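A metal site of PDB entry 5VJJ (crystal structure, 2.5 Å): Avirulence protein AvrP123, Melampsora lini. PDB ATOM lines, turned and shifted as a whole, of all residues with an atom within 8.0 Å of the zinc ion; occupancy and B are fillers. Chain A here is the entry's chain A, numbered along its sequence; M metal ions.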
ATOM      1  N   VAL A  14     -29.562   1.125   4.675  1.00  0.00           N
ATOM      2  CA  VAL A  14     -29.835  -0.313   4.635  1.00  0.00           C
ATOM      3  C   VAL A  14     -28.577  -1.045   5.066  1.00  0.00           C
ATOM      4  O   VAL A  14     -27.458  -0.537   4.978  1.00  0.00           O
ATOM      5  CB  VAL A  14     -30.286  -0.757   3.219  1.00  0.00           C
ATOM      6  CG1 VAL A  14     -29.150  -0.639   2.205  1.00  0.00           C
ATOM      7  CG2 VAL A  14     -30.843  -2.162   3.244  1.00  0.00           C
ATOM      8  N   GLN A  15     -28.769  -2.266   5.554  1.00  0.00           N
ATOM      9  CA  GLN A  15     -27.649  -3.143   5.866  1.00  0.00           C
ATOM     10  C   GLN A  15     -27.196  -3.856   4.593  1.00  0.00           C
ATOM     11  O   GLN A  15     -27.980  -4.539   3.941  1.00  0.00           O
ATOM     12  CB  GLN A  15     -28.049  -4.157   6.935  1.00  0.00           C
ATOM     13  CG  GLN A  15     -26.890  -5.003   7.433  1.00  0.00           C
ATOM     14  CD  GLN A  15     -27.163  -5.668   8.770  1.00  0.00           C
ATOM     15  OE1 GLN A  15     -28.305  -6.031   9.077  1.00  0.00           O
ATOM     16  NE2 GLN A  15     -26.123  -5.815   9.581  1.00  0.00           N
ATOM     17  N   CYS A  16     -25.927  -3.667   4.230  1.00  0.00           N
ATOM     18  CA  CYS A  16     -25.360  -4.361   3.089  1.00  0.00           C
ATOM     19  C   CYS A  16     -25.191  -5.845   3.415  1.00  0.00           C
ATOM     20  O   CYS A  16     -25.254  -6.262   4.571  1.00  0.00           O
ATOM     21  CB  CYS A  16     -24.005  -3.739   2.710  1.00  0.00           C
ATOM     22  SG  CYS A  16     -23.084  -4.609   1.398  1.00  0.00           S
ATOM     23  N   LEU A  17     -24.995  -6.644   2.369  1.00  0.00           N
ATOM     24  CA  LEU A  17     -24.786  -8.074   2.586  1.00  0.00           C
ATOM     25  C   LEU A  17     -23.552  -8.347   3.434  1.00  0.00           C
ATOM     26  O   LEU A  17     -23.484  -9.389   4.089  1.00  0.00           O
ATOM     27  CB  LEU A  17     -24.683  -8.791   1.247  1.00  0.00           C
ATOM     28  CG  LEU A  17     -25.940  -8.738   0.383  1.00  0.00           C
ATOM     29  CD1 LEU A  17     -25.651  -9.323  -0.995  1.00  0.00           C
ATOM     30  CD2 LEU A  17     -27.083  -9.478   1.053  1.00  0.00           C
ATOM     31  N   CYS A  18     -22.578  -7.445   3.409  1.00  0.00           N
ATOM     32  CA  CYS A  18     -21.436  -7.557   4.315  1.00  0.00           C
ATOM     33  C   CYS A  18     -21.775  -7.131   5.744  1.00  0.00           C
ATOM     34  O   CYS A  18     -20.903  -7.207   6.613  1.00  0.00           O
ATOM     35  CB  CYS A  18     -20.269  -6.718   3.790  1.00  0.00           C
ATOM     36  SG  CYS A  18     -20.425  -4.943   4.093  1.00  0.00           S
ATOM     37  N   ARG A  19     -23.009  -6.683   5.978  1.00  0.00           N
ATOM     38  CA  ARG A  19     -23.613  -6.325   7.255  1.00  0.00           C
ATOM     39  C   ARG A  19     -23.327  -4.884   7.663  1.00  0.00           C
ATOM     40  O   ARG A  19     -23.885  -4.418   8.654  1.00  0.00           O
ATOM     41  CB  ARG A  19     -23.209  -7.272   8.406  1.00  0.00           C
ATOM     42  CG  ARG A  19     -23.752  -8.673   8.238  1.00  0.00           C
ATOM     43  CD  ARG A  19     -23.550  -9.551   9.470  1.00  0.00           C
ATOM     44  NE  ARG A  19     -22.171 -10.038   9.597  1.00  0.00           N
ATOM     45  CZ  ARG A  19     -21.271  -9.577  10.465  1.00  0.00           C
ATOM     46  NH1 ARG A  19     -21.582  -8.608  11.324  1.00  0.00           N
ATOM     47  NH2 ARG A  19     -20.056 -10.104  10.485  1.00  0.00           N
ATOM     48  N   ARG A  20     -22.492  -4.143   6.926  1.00  0.00           N
ATOM     49  CA  ARG A  20     -22.306  -2.732   7.208  1.00  0.00           C
ATOM     50  C   ARG A  20     -23.555  -1.946   6.817  1.00  0.00           C
ATOM     51  O   ARG A  20     -24.364  -2.382   5.994  1.00  0.00           O
ATOM     52  CB  ARG A  20     -21.093  -2.178   6.466  1.00  0.00           C
ATOM     53  CG  ARG A  20     -19.761  -2.585   7.063  1.00  0.00           C
ATOM     54  CD  ARG A  20     -18.623  -2.215   6.142  1.00  0.00           C
ATOM     55  NE  ARG A  20     -17.318  -2.588   6.702  1.00  0.00           N
ATOM     56  CZ  ARG A  20     -16.727  -3.754   6.511  1.00  0.00           C
ATOM     57  NH1 ARG A  20     -17.300  -4.690   5.766  1.00  0.00           N
ATOM     58  NH2 ARG A  20     -15.540  -3.986   7.062  1.00  0.00           N
ATOM     59  N   ILE A  21     -23.697  -0.762   7.399  1.00  0.00           N
ATOM     60  CA  ILE A  21     -24.814   0.117   7.065  1.00  0.00           C
ATOM     61  C   ILE A  21     -24.429   0.942   5.846  1.00  0.00           C
ATOM     62  O   ILE A  21     -23.365   1.572   5.805  1.00  0.00           O
ATOM     63  CB  ILE A  21     -25.179   1.016   8.265  1.00  0.00           C
ATOM     64  CG1 ILE A  21     -25.493   0.162   9.499  1.00  0.00           C
ATOM     65  CG2 ILE A  21     -26.354   1.914   7.922  1.00  0.00           C
ATOM     66  CD1 ILE A  21     -26.625  -0.851   9.309  1.00  0.00           C
ATOM     67  N   ALA A  22     -25.295   0.929   4.837  1.00  0.00           N
ATOM     68  CA  ALA A  22     -25.037   1.606   3.576  1.00  0.00           C
ATOM     69  C   ALA A  22     -26.162   2.571   3.256  1.00  0.00           C
ATOM     70  O   ALA A  22     -27.319   2.330   3.619  1.00  0.00           O
ATOM     71  CB  ALA A  22     -24.888   0.602   2.430  1.00  0.00           C
ATOM     72  N   TYR A  56     -27.649   0.678  -3.149  1.00  0.00           N
ATOM     73  CA  TYR A  56     -26.915   1.438  -2.154  1.00  0.00           C
ATOM     74  C   TYR A  56     -25.439   1.487  -2.535  1.00  0.00           C
ATOM     75  O   TYR A  56     -24.994   0.828  -3.480  1.00  0.00           O
ATOM     76  CB  TYR A  56     -27.102   0.846  -0.758  1.00  0.00           C
ATOM     77  CG  TYR A  56     -26.932  -0.652  -0.725  1.00  0.00           C
ATOM     78  CD1 TYR A  56     -28.013  -1.508  -0.877  1.00  0.00           C
ATOM     79  CD2 TYR A  56     -25.673  -1.217  -0.544  1.00  0.00           C
ATOM     80  CE1 TYR A  56     -27.852  -2.878  -0.842  1.00  0.00           C
ATOM     81  CE2 TYR A  56     -25.506  -2.575  -0.503  1.00  0.00           C
ATOM     82  CZ  TYR A  56     -26.594  -3.410  -0.654  1.00  0.00           C
ATOM     83  OH  TYR A  56     -26.424  -4.777  -0.617  1.00  0.00           O
ATOM     84  N   ARG A  57     -24.685   2.290  -1.792  1.00  0.00           N
ATOM     85  CA  ARG A  57     -23.267   2.513  -2.005  1.00  0.00           C
ATOM     86  C   ARG A  57     -22.560   2.201  -0.688  1.00  0.00           C
ATOM     87  O   ARG A  57     -22.447   3.074   0.168  1.00  0.00           O
ATOM     88  CB  ARG A  57     -22.999   3.946  -2.471  1.00  0.00           C
ATOM     89  CG  ARG A  57     -21.532   4.277  -2.752  1.00  0.00           C
ATOM     90  CD  ARG A  57     -21.143   3.891  -4.173  1.00  0.00           C
ATOM     91  NE  ARG A  57     -21.663   4.833  -5.161  1.00  0.00           N
ATOM     92  CZ  ARG A  57     -20.963   5.839  -5.688  1.00  0.00           C
ATOM     93  NH1 ARG A  57     -19.700   6.052  -5.351  1.00  0.00           N
ATOM     94  NH2 ARG A  57     -21.542   6.627  -6.575  1.00  0.00           N
ATOM     95  N   CYS A  58     -22.096   0.960  -0.538  1.00  0.00           N
ATOM     96  CA  CYS A  58     -21.507   0.545   0.728  1.00  0.00           C
ATOM     97  C   CYS A  58     -20.125   1.178   0.903  1.00  0.00           C
ATOM     98  O   CYS A  58     -19.312   1.151  -0.040  1.00  0.00           O
ATOM     99  CB  CYS A  58     -21.376  -0.972   0.786  1.00  0.00           C
ATOM    100  SG  CYS A  58     -20.682  -1.573   2.344  1.00  0.00           S
ATOM    101  N   PRO A  59     -19.816   1.738   2.080  1.00  0.00           N
ATOM    102  CA  PRO A  59     -18.467   2.304   2.265  1.00  0.00           C
ATOM    103  C   PRO A  59     -17.360   1.282   2.074  1.00  0.00           C
ATOM    104  O   PRO A  59     -16.238   1.657   1.729  1.00  0.00           O
ATOM    105  CB  PRO A  59     -18.497   2.815   3.717  1.00  0.00           C
ATOM    106  CG  PRO A  59     -19.550   1.996   4.373  1.00  0.00           C
ATOM    107  CD  PRO A  59     -20.599   1.780   3.316  1.00  0.00           C
ATOM    108  N   ASN A  60     -17.656   0.007   2.285  1.00  0.00           N
ATOM    109  CA  ASN A  60     -16.689  -1.064   2.062  1.00  0.00           C
ATOM    110  C   ASN A  60     -16.780  -1.601   0.636  1.00  0.00           C
ATOM    111  O   ASN A  60     -15.785  -1.589  -0.099  1.00  0.00           O
ATOM    112  CB  ASN A  60     -16.919  -2.185   3.075  1.00  0.00           C
ATOM    113  CG  ASN A  60     -15.938  -3.329   2.925  1.00  0.00           C
ATOM    114  OD1 ASN A  60     -14.776  -3.206   3.285  1.00  0.00           O
ATOM    115  ND2 ASN A  60     -16.418  -4.443   2.386  1.00  0.00           N
ATOM    116  N   CYS A  61     -17.954  -2.067   0.247  1.00  0.00           N
ATOM    117  CA  CYS A  61     -18.141  -2.767  -1.025  1.00  0.00           C
ATOM    118  C   CYS A  61     -18.365  -1.841  -2.207  1.00  0.00           C
ATOM    119  O   CYS A  61     -18.337  -2.310  -3.349  1.00  0.00           O
ATOM    120  CB  CYS A  61     -19.329  -3.727  -0.921  1.00  0.00           C
ATOM    121  SG  CYS A  61     -19.395  -4.678   0.592  1.00  0.00           S
ATOM    122  N   GLY A  62     -18.599  -0.549  -1.985  1.00  0.00           N
ATOM    123  CA  GLY A  62     -18.980   0.328  -3.061  1.00  0.00           C
ATOM    124  C   GLY A  62     -20.356  -0.010  -3.599  1.00  0.00           C
ATOM    125  O   GLY A  62     -21.144  -0.701  -2.940  1.00  0.00           O
ATOM    126  N   PRO A  63     -20.673   0.459  -4.813  1.00  0.00           N
ATOM    127  CA  PRO A  63     -22.007   0.201  -5.377  1.00  0.00           C
ATOM    128  C   PRO A  63     -22.429  -1.251  -5.305  1.00  0.00           C
ATOM    129  O   PRO A  63     -21.731  -2.124  -5.807  1.00  0.00           O
ATOM    130  CB  PRO A  63     -21.856   0.670  -6.840  1.00  0.00           C
ATOM    131  CG  PRO A  63     -20.732   1.675  -6.813  1.00  0.00           C
ATOM    132  CD  PRO A  63     -19.803   1.226  -5.719  1.00  0.00           C
ATOM    133  N   ARG A  64     -23.578  -1.526  -4.686  1.00  0.00           N
ATOM    134  CA  ARG A  64     -24.044  -2.901  -4.545  1.00  0.00           C
ATOM    135  C   ARG A  64     -25.569  -2.912  -4.438  1.00  0.00           C
ATOM    136  O   ARG A  64     -26.199  -1.882  -4.184  1.00  0.00           O
ATOM    137  CB  ARG A  64     -23.416  -3.585  -3.316  1.00  0.00           C
ATOM    138  CG  ARG A  64     -23.616  -5.091  -3.271  1.00  0.00           C
ATOM    139  CD  ARG A  64     -22.813  -5.742  -2.169  1.00  0.00           C
ATOM    140  NE  ARG A  64     -22.864  -7.197  -2.240  1.00  0.00           N
ATOM    141  CZ  ARG A  64     -22.198  -8.024  -1.435  1.00  0.00           C
ATOM    142  NH1 ARG A  64     -21.404  -7.530  -0.487  1.00  0.00           N
ATOM    143  NH2 ARG A  64     -22.319  -9.335  -1.572  1.00  0.00           N
HETATM  144 ZN    ZN M   1     -20.927  -3.889   2.068  1.00  0.00          ZN
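ND2 of Asn 60 lies close to SG of Cys 61 (3.5 Å). The side-chain sulfur (SG) of Cys 58 sits close to the backbone NH (N) of Asn 60 (3.4 Å). The side-chain sulfur of Cys 18 lies close to the guanidinium group of Arg 20 (3.6 Å). SG of Cys 61 lies close to NH1 of Arg 64 (3.7 Å).
Of the 18 residues printed, 4 come within 4 Å of the zinc ion.
SG of Cys 61 is bound to the zinc ion (2.3 Å). The zinc ion is bound by SG of Cys 18 (2.3 Å). The zinc ion is bound by SG of Cys 58 (2.3 Å). The zinc ion is bound by SG of Cys 16 (2.4 Å).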
